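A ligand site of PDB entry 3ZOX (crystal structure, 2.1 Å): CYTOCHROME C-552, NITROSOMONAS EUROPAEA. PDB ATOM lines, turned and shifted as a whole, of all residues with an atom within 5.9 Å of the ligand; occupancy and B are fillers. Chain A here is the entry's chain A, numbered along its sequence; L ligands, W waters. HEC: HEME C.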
ATOM      1  N   ALA A   5     -25.882  11.014  -7.591  1.00  0.00           N
ATOM      2  CA  ALA A   5     -25.620  10.620  -8.980  1.00  0.00           C
ATOM      3  C   ALA A   5     -25.681  11.836  -9.908  1.00  0.00           C
ATOM      4  O   ALA A   5     -24.811  12.013 -10.762  1.00  0.00           O
ATOM      5  CB  ALA A   5     -26.621   9.579  -9.435  1.00  0.00           C
ATOM      6  N   ASN A   8     -22.726  14.073  -9.699  1.00  0.00           N
ATOM      7  CA  ASN A   8     -21.515  13.540 -10.235  1.00  0.00           C
ATOM      8  C   ASN A   8     -21.610  13.165 -11.699  1.00  0.00           C
ATOM      9  O   ASN A   8     -20.786  12.416 -12.178  1.00  0.00           O
ATOM     10  CB  ASN A   8     -21.007  12.394  -9.368  1.00  0.00           C
ATOM     11  CG  ASN A   8     -20.497  12.874  -8.027  1.00  0.00           C
ATOM     12  OD1 ASN A   8     -21.073  12.579  -6.993  1.00  0.00           O
ATOM     13  ND2 ASN A   8     -19.431  13.661  -8.059  1.00  0.00           N
ATOM     14  N   ASN A   9     -22.596  13.731 -12.375  1.00  0.00           N
ATOM     15  CA  ASN A   9     -22.930  13.465 -13.771  1.00  0.00           C
ATOM     16  C   ASN A   9     -23.121  12.038 -14.240  1.00  0.00           C
ATOM     17  O   ASN A   9     -22.918  11.712 -15.413  1.00  0.00           O
ATOM     18  CB  ASN A   9     -22.063  14.298 -14.703  1.00  0.00           C
ATOM     19  CG  ASN A   9     -22.585  15.707 -14.841  1.00  0.00           C
ATOM     20  OD1 ASN A   9     -23.493  15.995 -15.665  1.00  0.00           O
ATOM     21  ND2 ASN A   9     -22.096  16.585 -13.989  1.00  0.00           N
ATOM     22  N   CYS A  10     -23.565  11.200 -13.332  1.00  0.00           N
ATOM     23  CA  CYS A  10     -23.965   9.881 -13.694  1.00  0.00           C
ATOM     24  C   CYS A  10     -25.093   9.927 -14.674  1.00  0.00           C
ATOM     25  O   CYS A  10     -25.200   9.044 -15.559  1.00  0.00           O
ATOM     26  CB  CYS A  10     -24.381   9.069 -12.412  1.00  0.00           C
ATOM     27  SG  CYS A  10     -22.990   9.174 -11.250  1.00  0.00           S
ATOM     28  N   ILE A  11     -25.986  10.894 -14.463  1.00  0.00           N
ATOM     29  CA  ILE A  11     -27.273  10.931 -15.134  1.00  0.00           C
ATOM     30  C   ILE A  11     -27.101  11.431 -16.571  1.00  0.00           C
ATOM     31  O   ILE A  11     -27.986  11.280 -17.437  1.00  0.00           O
ATOM     32  CB  ILE A  11     -28.314  11.766 -14.302  1.00  0.00           C
ATOM     33  CG1 ILE A  11     -28.498  11.190 -12.857  1.00  0.00           C
ATOM     34  CG2 ILE A  11     -29.685  11.822 -14.973  1.00  0.00           C
ATOM     35  CD1 ILE A  11     -28.701   9.679 -12.782  1.00  0.00           C
ATOM     36  N   ALA A  12     -25.960  12.039 -16.856  1.00  0.00           N
ATOM     37  CA  ALA A  12     -25.770  12.447 -18.231  1.00  0.00           C
ATOM     38  C   ALA A  12     -25.652  11.225 -19.128  1.00  0.00           C
ATOM     39  O   ALA A  12     -25.983  11.286 -20.339  1.00  0.00           O
ATOM     40  CB  ALA A  12     -24.553  13.346 -18.343  1.00  0.00           C
ATOM     41  N   CYS A  13     -25.220  10.083 -18.565  1.00  0.00           N
ATOM     42  CA  CYS A  13     -25.052   8.840 -19.372  1.00  0.00           C
ATOM     43  C   CYS A  13     -25.966   7.688 -18.961  1.00  0.00           C
ATOM     44  O   CYS A  13     -26.150   6.740 -19.734  1.00  0.00           O
ATOM     45  CB  CYS A  13     -23.599   8.357 -19.378  1.00  0.00           C
ATOM     46  SG  CYS A  13     -22.387   9.515 -20.111  1.00  0.00           S
ATOM     47  N   HIS A  14     -26.491   7.741 -17.738  1.00  0.00           N
ATOM     48  CA  HIS A  14     -27.359   6.713 -17.229  1.00  0.00           C
ATOM     49  C   HIS A  14     -28.744   7.266 -16.841  1.00  0.00           C
ATOM     50  O   HIS A  14     -28.830   8.319 -16.210  1.00  0.00           O
ATOM     51  CB  HIS A  14     -26.719   6.154 -15.969  1.00  0.00           C
ATOM     52  CG  HIS A  14     -25.414   5.423 -16.174  1.00  0.00           C
ATOM     53  ND1 HIS A  14     -25.359   4.097 -16.522  1.00  0.00           N
ATOM     54  CD2 HIS A  14     -24.136   5.817 -16.020  1.00  0.00           C
ATOM     55  CE1 HIS A  14     -24.096   3.713 -16.583  1.00  0.00           C
ATOM     56  NE2 HIS A  14     -23.329   4.728 -16.256  1.00  0.00           N
ATOM     57  N   VAL A  21     -26.631   6.143 -22.703  1.00  0.00           N
ATOM     58  CA  VAL A  21     -25.314   5.738 -23.184  1.00  0.00           C
ATOM     59  C   VAL A  21     -24.833   4.498 -22.403  1.00  0.00           C
ATOM     60  O   VAL A  21     -24.487   3.467 -23.031  1.00  0.00           O
ATOM     61  CB  VAL A  21     -24.266   6.879 -23.144  1.00  0.00           C
ATOM     62  CG1 VAL A  21     -22.867   6.344 -23.495  1.00  0.00           C
ATOM     63  CG2 VAL A  21     -24.683   8.076 -24.030  1.00  0.00           C
ATOM     64  N   GLY A  22     -24.829   4.584 -21.073  1.00  0.00           N
ATOM     65  CA  GLY A  22     -24.505   3.436 -20.190  1.00  0.00           C
ATOM     66  C   GLY A  22     -25.796   2.662 -19.958  1.00  0.00           C
ATOM     67  O   GLY A  22     -26.900   3.169 -20.301  1.00  0.00           O
ATOM     68  N   PRO A  23     -25.693   1.441 -19.402  1.00  0.00           N
ATOM     69  CA  PRO A  23     -26.866   0.646 -19.082  1.00  0.00           C
ATOM     70  C   PRO A  23     -27.829   1.371 -18.096  1.00  0.00           C
ATOM     71  O   PRO A  23     -27.428   2.301 -17.350  1.00  0.00           O
ATOM     72  CB  PRO A  23     -26.282  -0.576 -18.351  1.00  0.00           C
ATOM     73  CG  PRO A  23     -24.926  -0.180 -17.905  1.00  0.00           C
ATOM     74  CD  PRO A  23     -24.457   0.824 -18.901  1.00  0.00           C
ATOM     75  N   LEU A  25     -29.528   2.111 -14.829  1.00  0.00           N
ATOM     76  CA  LEU A  25     -29.225   1.774 -13.400  1.00  0.00           C
ATOM     77  C   LEU A  25     -29.937   0.517 -12.844  1.00  0.00           C
ATOM     78  O   LEU A  25     -29.283  -0.344 -12.220  1.00  0.00           O
ATOM     79  CB  LEU A  25     -29.419   2.995 -12.447  1.00  0.00           C
ATOM     80  CG  LEU A  25     -28.464   4.139 -12.871  1.00  0.00           C
ATOM     81  CD1 LEU A  25     -28.445   5.319 -11.918  1.00  0.00           C
ATOM     82  CD2 LEU A  25     -27.059   3.626 -13.169  1.00  0.00           C
ATOM     83  N   ILE A  28     -28.326  -2.671 -14.073  1.00  0.00           N
ATOM     84  CA  ILE A  28     -27.150  -2.943 -13.263  1.00  0.00           C
ATOM     85  C   ILE A  28     -27.523  -3.530 -11.929  1.00  0.00           C
ATOM     86  O   ILE A  28     -26.937  -4.547 -11.553  1.00  0.00           O
ATOM     87  CB  ILE A  28     -26.251  -1.688 -13.044  1.00  0.00           C
ATOM     88  CG1 ILE A  28     -25.795  -1.128 -14.398  1.00  0.00           C
ATOM     89  CG2 ILE A  28     -24.994  -2.035 -12.238  1.00  0.00           C
ATOM     90  CD1 ILE A  28     -25.356   0.324 -14.339  1.00  0.00           C
ATOM     91  N   LYS A  31     -28.563  -7.232 -12.593  1.00  0.00           N
ATOM     92  CA  LYS A  31     -27.490  -8.125 -13.019  1.00  0.00           C
ATOM     93  C   LYS A  31     -26.696  -8.639 -11.792  1.00  0.00           C
ATOM     94  O   LYS A  31     -26.305  -9.793 -11.698  1.00  0.00           O
ATOM     95  CB  LYS A  31     -26.540  -7.359 -13.935  1.00  0.00           C
ATOM     96  CG  LYS A  31     -25.437  -8.234 -14.515  1.00  0.00           C
ATOM     97  CD  LYS A  31     -24.590  -7.508 -15.595  1.00  0.00           C
ATOM     98  CE  LYS A  31     -23.503  -8.423 -16.158  1.00  0.00           C
ATOM     99  NZ  LYS A  31     -24.150  -9.651 -16.681  1.00  0.00           N
ATOM    100  N   TYR A  32     -26.350  -7.696 -10.939  1.00  0.00           N
ATOM    101  CA  TYR A  32     -25.503  -7.971  -9.789  1.00  0.00           C
ATOM    102  C   TYR A  32     -26.299  -8.205  -8.463  1.00  0.00           C
ATOM    103  O   TYR A  32     -25.701  -8.321  -7.440  1.00  0.00           O
ATOM    104  CB  TYR A  32     -24.479  -6.854  -9.637  1.00  0.00           C
ATOM    105  CG  TYR A  32     -23.651  -6.604 -10.883  1.00  0.00           C
ATOM    106  CD1 TYR A  32     -22.671  -7.572 -11.294  1.00  0.00           C
ATOM    107  CD2 TYR A  32     -23.842  -5.453 -11.679  1.00  0.00           C
ATOM    108  CE1 TYR A  32     -21.920  -7.373 -12.445  1.00  0.00           C
ATOM    109  CE2 TYR A  32     -23.096  -5.250 -12.845  1.00  0.00           C
ATOM    110  CZ  TYR A  32     -22.125  -6.219 -13.202  1.00  0.00           C
ATOM    111  OH  TYR A  32     -21.360  -6.044 -14.338  1.00  0.00           O
ATOM    112  N   TYR A  41     -17.329  -4.388  -6.080  1.00  0.00           N
ATOM    113  CA  TYR A  41     -17.140  -4.564  -7.518  1.00  0.00           C
ATOM    114  C   TYR A  41     -17.631  -3.299  -8.208  1.00  0.00           C
ATOM    115  O   TYR A  41     -16.906  -2.739  -9.003  1.00  0.00           O
ATOM    116  CB  TYR A  41     -17.950  -5.743  -8.067  1.00  0.00           C
ATOM    117  CG  TYR A  41     -17.965  -5.737  -9.595  1.00  0.00           C
ATOM    118  CD1 TYR A  41     -16.878  -6.207 -10.327  1.00  0.00           C
ATOM    119  CD2 TYR A  41     -19.070  -5.281 -10.304  1.00  0.00           C
ATOM    120  CE1 TYR A  41     -16.901  -6.233 -11.744  1.00  0.00           C
ATOM    121  CE2 TYR A  41     -19.107  -5.307 -11.715  1.00  0.00           C
ATOM    122  CZ  TYR A  41     -18.008  -5.793 -12.437  1.00  0.00           C
ATOM    123  OH  TYR A  41     -18.030  -5.787 -13.828  1.00  0.00           O
ATOM    124  N   LEU A  42     -18.875  -2.895  -7.947  1.00  0.00           N
ATOM    125  CA  LEU A  42     -19.399  -1.631  -8.547  1.00  0.00           C
ATOM    126  C   LEU A  42     -18.632  -0.357  -8.202  1.00  0.00           C
ATOM    127  O   LEU A  42     -18.363   0.491  -9.069  1.00  0.00           O
ATOM    128  CB  LEU A  42     -20.891  -1.414  -8.241  1.00  0.00           C
ATOM    129  CG  LEU A  42     -21.742  -2.561  -8.855  1.00  0.00           C
ATOM    130  CD1 LEU A  42     -23.194  -2.359  -8.524  1.00  0.00           C
ATOM    131  CD2 LEU A  42     -21.542  -2.704 -10.380  1.00  0.00           C
ATOM    132  N   LYS A  45     -15.687  -0.183 -10.436  1.00  0.00           N
ATOM    133  CA  LYS A  45     -16.017   0.213 -11.816  1.00  0.00           C
ATOM    134  C   LYS A  45     -16.324   1.666 -11.910  1.00  0.00           C
ATOM    135  O   LYS A  45     -16.013   2.309 -12.921  1.00  0.00           O
ATOM    136  CB  LYS A  45     -17.204  -0.599 -12.413  1.00  0.00           C
ATOM    137  CG  LYS A  45     -17.009  -2.086 -12.466  1.00  0.00           C
ATOM    138  CD  LYS A  45     -15.596  -2.582 -12.858  1.00  0.00           C
ATOM    139  CE  LYS A  45     -15.363  -2.837 -14.377  1.00  0.00           C
ATOM    140  NZ  LYS A  45     -16.492  -3.370 -15.247  1.00  0.00           N
ATOM    141  N   ILE A  46     -16.963   2.225 -10.874  1.00  0.00           N
ATOM    142  CA  ILE A  46     -17.359   3.634 -10.904  1.00  0.00           C
ATOM    143  C   ILE A  46     -16.116   4.529 -10.875  1.00  0.00           C
ATOM    144  O   ILE A  46     -16.001   5.491 -11.669  1.00  0.00           O
ATOM    145  CB  ILE A  46     -18.295   3.965  -9.716  1.00  0.00           C
ATOM    146  CG1 ILE A  46     -19.650   3.285  -9.894  1.00  0.00           C
ATOM    147  CG2 ILE A  46     -18.370   5.483  -9.476  1.00  0.00           C
ATOM    148  CD1 ILE A  46     -20.425   3.214  -8.554  1.00  0.00           C
ATOM    149  N   SER A  50     -14.910   1.257 -17.001  1.00  0.00           N
ATOM    150  CA  SER A  50     -15.466  -0.041 -17.411  1.00  0.00           C
ATOM    151  C   SER A  50     -15.421  -0.147 -18.942  1.00  0.00           C
ATOM    152  O   SER A  50     -15.572   0.857 -19.659  1.00  0.00           O
ATOM    153  CB  SER A  50     -16.924  -0.123 -16.943  1.00  0.00           C
ATOM    154  OG  SER A  50     -17.505  -1.400 -17.129  1.00  0.00           O
ATOM    155  N   SER A  51     -15.259  -1.352 -19.440  1.00  0.00           N
ATOM    156  CA  SER A  51     -15.159  -1.597 -20.853  1.00  0.00           C
ATOM    157  C   SER A  51     -15.640  -3.004 -21.132  1.00  0.00           C
ATOM    158  O   SER A  51     -15.130  -3.951 -20.527  1.00  0.00           O
ATOM    159  CB  SER A  51     -13.697  -1.425 -21.291  1.00  0.00           C
ATOM    160  OG  SER A  51     -13.463  -1.982 -22.558  1.00  0.00           O
ATOM    161  N   GLY A  52     -16.628  -3.127 -22.046  1.00  0.00           N
ATOM    162  CA  GLY A  52     -17.011  -4.429 -22.614  1.00  0.00           C
ATOM    163  C   GLY A  52     -18.157  -5.155 -21.922  1.00  0.00           C
ATOM    164  O   GLY A  52     -18.667  -6.154 -22.501  1.00  0.00           O
ATOM    165  N   VAL A  53     -18.586  -4.679 -20.722  1.00  0.00           N
ATOM    166  CA  VAL A  53     -19.576  -5.432 -19.945  1.00  0.00           C
ATOM    167  C   VAL A  53     -20.976  -5.317 -20.592  1.00  0.00           C
ATOM    168  O   VAL A  53     -21.748  -6.246 -20.626  1.00  0.00           O
ATOM    169  CB  VAL A  53     -19.626  -4.976 -18.463  1.00  0.00           C
ATOM    170  CG1 VAL A  53     -20.647  -5.819 -17.706  1.00  0.00           C
ATOM    171  CG2 VAL A  53     -18.286  -5.128 -17.774  1.00  0.00           C
ATOM    172  N   TRP A  54     -21.274  -4.141 -21.124  1.00  0.00           N
ATOM    173  CA  TRP A  54     -22.578  -3.823 -21.664  1.00  0.00           C
ATOM    174  C   TRP A  54     -22.703  -3.490 -23.120  1.00  0.00           C
ATOM    175  O   TRP A  54     -23.827  -3.230 -23.554  1.00  0.00           O
ATOM    176  CB  TRP A  54     -23.208  -2.662 -20.868  1.00  0.00           C
ATOM    177  CG  TRP A  54     -23.419  -3.061 -19.355  1.00  0.00           C
ATOM    178  CD1 TRP A  54     -22.539  -2.892 -18.312  1.00  0.00           C
ATOM    179  CD2 TRP A  54     -24.595  -3.672 -18.797  1.00  0.00           C
ATOM    180  NE1 TRP A  54     -23.123  -3.369 -17.105  1.00  0.00           N
ATOM    181  CE2 TRP A  54     -24.391  -3.815 -17.387  1.00  0.00           C
ATOM    182  CE3 TRP A  54     -25.852  -4.024 -19.336  1.00  0.00           C
ATOM    183  CZ2 TRP A  54     -25.360  -4.356 -16.555  1.00  0.00           C
ATOM    184  CZ3 TRP A  54     -26.816  -4.559 -18.491  1.00  0.00           C
ATOM    185  CH2 TRP A  54     -26.551  -4.741 -17.121  1.00  0.00           C
ATOM    186  N   GLY A  55     -21.595  -3.440 -23.875  1.00  0.00           N
ATOM    187  CA  GLY A  55     -21.612  -2.955 -25.272  1.00  0.00           C
ATOM    188  C   GLY A  55     -20.242  -2.383 -25.630  1.00  0.00           C
ATOM    189  O   GLY A  55     -19.264  -2.677 -24.955  1.00  0.00           O
ATOM    190  N   GLN A  56     -20.117  -1.635 -26.709  1.00  0.00           N
ATOM    191  CA  GLN A  56     -18.771  -1.149 -27.109  1.00  0.00           C
ATOM    192  C   GLN A  56     -18.328   0.184 -26.487  1.00  0.00           C
ATOM    193  O   GLN A  56     -17.143   0.506 -26.529  1.00  0.00           O
ATOM    194  CB  GLN A  56     -18.479  -1.175 -28.651  1.00  0.00           C
ATOM    195  CG  GLN A  56     -19.599  -0.708 -29.568  1.00  0.00           C
ATOM    196  CD  GLN A  56     -19.182  -0.603 -31.081  1.00  0.00           C
ATOM    197  OE1 GLN A  56     -18.211  -1.184 -31.531  1.00  0.00           O
ATOM    198  NE2 GLN A  56     -19.951   0.150 -31.841  1.00  0.00           N
ATOM    199  N   ILE A  57     -19.244   0.990 -25.991  1.00  0.00           N
ATOM    200  CA  ILE A  57     -18.864   2.277 -25.431  1.00  0.00           C
ATOM    201  C   ILE A  57     -18.266   2.023 -24.026  1.00  0.00           C
ATOM    202  O   ILE A  57     -18.894   1.380 -23.180  1.00  0.00           O
ATOM    203  CB  ILE A  57     -20.102   3.246 -25.342  1.00  0.00           C
ATOM    204  CG1 ILE A  57     -20.779   3.350 -26.736  1.00  0.00           C
ATOM    205  CG2 ILE A  57     -19.702   4.621 -24.790  1.00  0.00           C
ATOM    206  CD1 ILE A  57     -21.950   4.305 -26.841  1.00  0.00           C
ATOM    207  N   PRO A  58     -17.023   2.500 -23.790  1.00  0.00           N
ATOM    208  CA  PRO A  58     -16.346   2.368 -22.491  1.00  0.00           C
ATOM    209  C   PRO A  58     -16.859   3.453 -21.555  1.00  0.00           C
ATOM    210  O   PRO A  58     -17.299   4.478 -22.025  1.00  0.00           O
ATOM    211  CB  PRO A  58     -14.899   2.727 -22.812  1.00  0.00           C
ATOM    212  CG  PRO A  58     -15.024   3.661 -23.979  1.00  0.00           C
ATOM    213  CD  PRO A  58     -16.152   3.112 -24.809  1.00  0.00           C
ATOM    214  N   MET A  59     -16.822   3.202 -20.261  1.00  0.00           N
ATOM    215  CA  MET A  59     -17.166   4.234 -19.284  1.00  0.00           C
ATOM    216  C   MET A  59     -15.834   4.772 -18.804  1.00  0.00           C
ATOM    217  O   MET A  59     -15.014   4.026 -18.393  1.00  0.00           O
ATOM    218  CB  MET A  59     -17.940   3.675 -18.095  1.00  0.00           C
ATOM    219  CG  MET A  59     -18.144   4.733 -16.978  1.00  0.00           C
ATOM    220  SD  MET A  59     -19.180   4.183 -15.607  1.00  0.00           S
ATOM    221  CE  MET A  59     -18.421   5.190 -14.307  1.00  0.00           C
ATOM    222  N   PRO A  60     -15.645   6.101 -18.837  1.00  0.00           N
ATOM    223  CA  PRO A  60     -14.413   6.651 -18.340  1.00  0.00           C
ATOM    224  C   PRO A  60     -14.396   6.560 -16.807  1.00  0.00           C
ATOM    225  O   PRO A  60     -15.461   6.489 -16.175  1.00  0.00           O
ATOM    226  CB  PRO A  60     -14.443   8.093 -18.864  1.00  0.00           C
ATOM    227  CG  PRO A  60     -15.898   8.420 -18.866  1.00  0.00           C
ATOM    228  CD  PRO A  60     -16.605   7.125 -19.234  1.00  0.00           C
ATOM    229  N   VAL A  62     -14.477   7.772 -13.200  1.00  0.00           N
ATOM    230  CA  VAL A  62     -15.060   9.024 -12.632  1.00  0.00           C
ATOM    231  C   VAL A  62     -14.375   9.395 -11.309  1.00  0.00           C
ATOM    232  O   VAL A  62     -14.212   8.555 -10.409  1.00  0.00           O
ATOM    233  CB  VAL A  62     -16.616   8.993 -12.506  1.00  0.00           C
ATOM    234  CG1 VAL A  62     -17.194  10.383 -12.189  1.00  0.00           C
ATOM    235  CG2 VAL A  62     -17.272   8.503 -13.810  1.00  0.00           C
ATOM    236  N   VAL A  64     -14.564  10.378  -8.166  1.00  0.00           N
ATOM    237  CA  VAL A  64     -15.296  10.568  -6.926  1.00  0.00           C
ATOM    238  C   VAL A  64     -14.405   9.998  -5.820  1.00  0.00           C
ATOM    239  O   VAL A  64     -13.522   9.169  -6.092  1.00  0.00           O
ATOM    240  CB  VAL A  64     -16.697   9.887  -6.952  1.00  0.00           C
ATOM    241  CG1 VAL A  64     -17.675  10.658  -7.853  1.00  0.00           C
ATOM    242  CG2 VAL A  64     -16.623   8.407  -7.368  1.00  0.00           C
ATOM    243  N   LEU A  72     -22.778   5.394  -4.015  1.00  0.00           N
ATOM    244  CA  LEU A  72     -23.456   5.285  -5.316  1.00  0.00           C
ATOM    245  C   LEU A  72     -23.652   3.823  -5.683  1.00  0.00           C
ATOM    246  O   LEU A  72     -24.721   3.472  -6.189  1.00  0.00           O
ATOM    247  CB  LEU A  72     -22.638   5.978  -6.411  1.00  0.00           C
ATOM    248  CG  LEU A  72     -22.742   7.490  -6.415  1.00  0.00           C
ATOM    249  CD1 LEU A  72     -21.666   8.088  -7.284  1.00  0.00           C
ATOM    250  CD2 LEU A  72     -24.133   7.879  -6.904  1.00  0.00           C
ATOM    251  N   ALA A  73     -22.658   2.974  -5.408  1.00  0.00           N
ATOM    252  CA  ALA A  73     -22.858   1.512  -5.615  1.00  0.00           C
ATOM    253  C   ALA A  73     -23.970   0.935  -4.758  1.00  0.00           C
ATOM    254  O   ALA A  73     -24.823   0.177  -5.223  1.00  0.00           O
ATOM    255  CB  ALA A  73     -21.560   0.757  -5.339  1.00  0.00           C
ATOM    256  N   ILE A  76     -27.297   2.162  -6.265  1.00  0.00           N
ATOM    257  CA  ILE A  76     -27.715   1.428  -7.489  1.00  0.00           C
ATOM    258  C   ILE A  76     -28.279   0.066  -7.116  1.00  0.00           C
ATOM    259  O   ILE A  76     -29.390  -0.332  -7.559  1.00  0.00           O
ATOM    260  CB  ILE A  76     -26.578   1.235  -8.497  1.00  0.00           C
ATOM    261  CG1 ILE A  76     -26.241   2.579  -9.170  1.00  0.00           C
ATOM    262  CG2 ILE A  76     -26.938   0.180  -9.541  1.00  0.00           C
ATOM    263  CD1 ILE A  76     -24.785   2.663  -9.605  1.00  0.00           C
HETATM  264 FE   HEC L   1     -21.366   4.553 -15.954  1.00  0.00          FE
HETATM  265  CHA HEC L   1     -21.262   1.266 -16.895  1.00  0.00           C
HETATM  266  CHB HEC L   1     -22.155   3.735 -12.856  1.00  0.00           C
HETATM  267  CHC HEC L   1     -20.871   7.947 -14.861  1.00  0.00           C
HETATM  268  CHD HEC L   1     -21.092   5.604 -19.158  1.00  0.00           C
HETATM  269  NA  HEC L   1     -21.635   2.782 -15.072  1.00  0.00           N
HETATM  270  C1A HEC L   1     -21.501   1.520 -15.565  1.00  0.00           C
HETATM  271  C2A HEC L   1     -21.703   0.546 -14.473  1.00  0.00           C
HETATM  272  C3A HEC L   1     -21.938   1.248 -13.357  1.00  0.00           C
HETATM  273  C4A HEC L   1     -21.903   2.680 -13.719  1.00  0.00           C
HETATM  274  CMA HEC L   1     -22.234   0.707 -11.943  1.00  0.00           C
HETATM  275  CAA HEC L   1     -21.665  -0.996 -14.595  1.00  0.00           C
HETATM  276  CBA HEC L   1     -20.241  -1.522 -14.694  1.00  0.00           C
HETATM  277  CGA HEC L   1     -20.259  -3.026 -14.729  1.00  0.00           C
HETATM  278  O1A HEC L   1     -21.306  -3.673 -14.896  1.00  0.00           O
HETATM  279  O2A HEC L   1     -19.166  -3.634 -14.625  1.00  0.00           O
HETATM  280  NB  HEC L   1     -21.486   5.677 -14.203  1.00  0.00           N
HETATM  281  C1B HEC L   1     -21.870   5.058 -13.050  1.00  0.00           C
HETATM  282  C2B HEC L   1     -21.947   6.069 -11.994  1.00  0.00           C
HETATM  283  C3B HEC L   1     -21.572   7.261 -12.518  1.00  0.00           C
HETATM  284  C4B HEC L   1     -21.287   7.026 -13.925  1.00  0.00           C
HETATM  285  CMB HEC L   1     -22.349   5.711 -10.541  1.00  0.00           C
HETATM  286  CAB HEC L   1     -21.447   8.627 -11.795  1.00  0.00           C
HETATM  287  CBB HEC L   1     -20.310   8.899 -11.136  1.00  0.00           C
HETATM  288  NC  HEC L   1     -21.050   6.445 -16.829  1.00  0.00           N
HETATM  289  C1C HEC L   1     -20.884   7.675 -16.215  1.00  0.00           C
HETATM  290  C2C HEC L   1     -20.710   8.651 -17.264  1.00  0.00           C
HETATM  291  C3C HEC L   1     -20.748   8.016 -18.452  1.00  0.00           C
HETATM  292  C4C HEC L   1     -20.951   6.594 -18.187  1.00  0.00           C
HETATM  293  CMC HEC L   1     -20.513  10.185 -16.990  1.00  0.00           C
HETATM  294  CAC HEC L   1     -20.689   8.646 -19.848  1.00  0.00           C
HETATM  295  CBC HEC L   1     -19.623   9.337 -20.301  1.00  0.00           C
HETATM  296  ND  HEC L   1     -21.235   3.561 -17.789  1.00  0.00           N
HETATM  297  C1D HEC L   1     -21.092   4.237 -18.973  1.00  0.00           C
HETATM  298  C2D HEC L   1     -20.938   3.238 -20.007  1.00  0.00           C
HETATM  299  C3D HEC L   1     -21.006   1.895 -19.308  1.00  0.00           C
HETATM  300  C4D HEC L   1     -21.175   2.198 -17.913  1.00  0.00           C
HETATM  301  CMD HEC L   1     -20.751   3.519 -21.504  1.00  0.00           C
HETATM  302  CAD HEC L   1     -20.847   0.505 -19.909  1.00  0.00           C
HETATM  303  CBD HEC L   1     -19.362   0.137 -19.833  1.00  0.00           C
HETATM  304  CGD HEC L   1     -19.191  -1.334 -20.158  1.00  0.00           C
HETATM  305  O1D HEC L   1     -18.437  -2.021 -19.416  1.00  0.00           O
HETATM  306  O2D HEC L   1     -19.813  -1.868 -21.130  1.00  0.00           O
HETATM  307  O   HOH W   1     -20.835  -0.217 -23.305  1.00  0.00           O
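O of Cys 13 lies within hydrogen-bond range of N of Gly 22 (2.9 Å).
The backbone NH of Val 62 lies within hydrogen-bond range of the backbone carbonyl oxygen of Ile 46, at 3.1 Å.
N of Cys 10 lies within hydrogen-bond range of O of Ala 5, 3.0 Å away.
OH of Tyr 32 is in hydrogen-bond range of OH of Tyr 41.
O of Cys 13 lies within hydrogen-bond range of N of Val 21 (3.1 Å).
The backbone carbonyl oxygen (O) of Pro 23 is in hydrogen-bond range of a ring nitrogen (ND1) of His 14 (2.9 Å).
The side-chain hydroxyl (OG) of Ser 50 lies within hydrogen-bond range of the side-chain amino group (NZ) of Lys 45, 2.9 Å away.
NZ of Lys 45 lies within hydrogen-bond range of OH of Tyr 41, 3.2 Å away.
Water W1 lies within hydrogen-bond range of the backbone carbonyl oxygen of Ile 57, an oxygen (O2D) of the ligand and the backbone carbonyl oxygen of Gly 55.
N of Gly 52 sits at hydrogen-bond distance from O1D of the ligand, at 3.4 Å.
NZ of Lys 45 lies within salt-bridge range of O2A of the ligand (2.8 Å).
An iron atom (FE) of the ligand is bound by the side-chain sulfur (SD) of Met 59 (2.2 Å).
N of Ser 51 lies within hydrogen-bond range of O1D of the ligand.
The side-chain sulfur of Cys 10 is covalently linked to a carbon (CAB) of the ligand, 1.7 Å away.
A ring nitrogen (NE2) of His 14 is bound to an iron atom (FE) of the ligand.
OH of Tyr 32 is in hydrogen-bond range of O1A of the ligand, 2.4 Å away.
OH of Tyr 41 is in hydrogen-bond range of O2A of the ligand, at 2.6 Å.
OG of Ser 50 sits at hydrogen-bond distance from O1D of the ligand (2.5 Å).
A carbon (CAC) of the ligand is covalently linked to the side-chain sulfur (SG) of Cys 13, 1.9 Å away.
O1D of the ligand is in hydrogen-bond range of N of Val 53, at 3.0 Å.
NE1 of Trp 54 lies within hydrogen-bond range of O1A of the ligand (2.9 Å).
The backbone NH of Trp 54 sits at hydrogen-bond distance from an oxygen (O2D) of the ligand (2.7 Å).
Merely in contact with the ligand: Asn 8 (3.7 Å), Asn 9 (3.3 Å), Gly 22 (3.6 Å), Pro 23 (3.6 Å), Ile 28 (3.7 Å), Leu 42 (3.8 Å), Ile 46 (3.7 Å), Gly 55 (3.6 Å), Ile 57 (3.3 Å), Pro 58 (3.6 Å), Pro 60 (3.9 Å), Val 62 (3.6 Å) and Ile 76 (3.97 Å).
Hydrophobic or aromatic side chains within 4 Å of the ligand: His 14, Pro 23, Ile 28, Tyr 32, Tyr 41, Leu 42, Ile 46, Val 53, Trp 54, Ile 57, Met 59, Pro 60, Val 62 and Ile 76.
Within 4 Å of the ligand: Asn 8, Asn 9, Cys 10, Cys 13, His 14, Gly 22, Pro 23, Ile 28, Tyr 32, Tyr 41, Leu 42, Lys 45, Ile 46, Ser 50, Ser 51, Gly 52, Val 53, Trp 54, Gly 55, Ile 57, Pro 58, Met 59, Pro 60, Val 62 and Ile 76.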
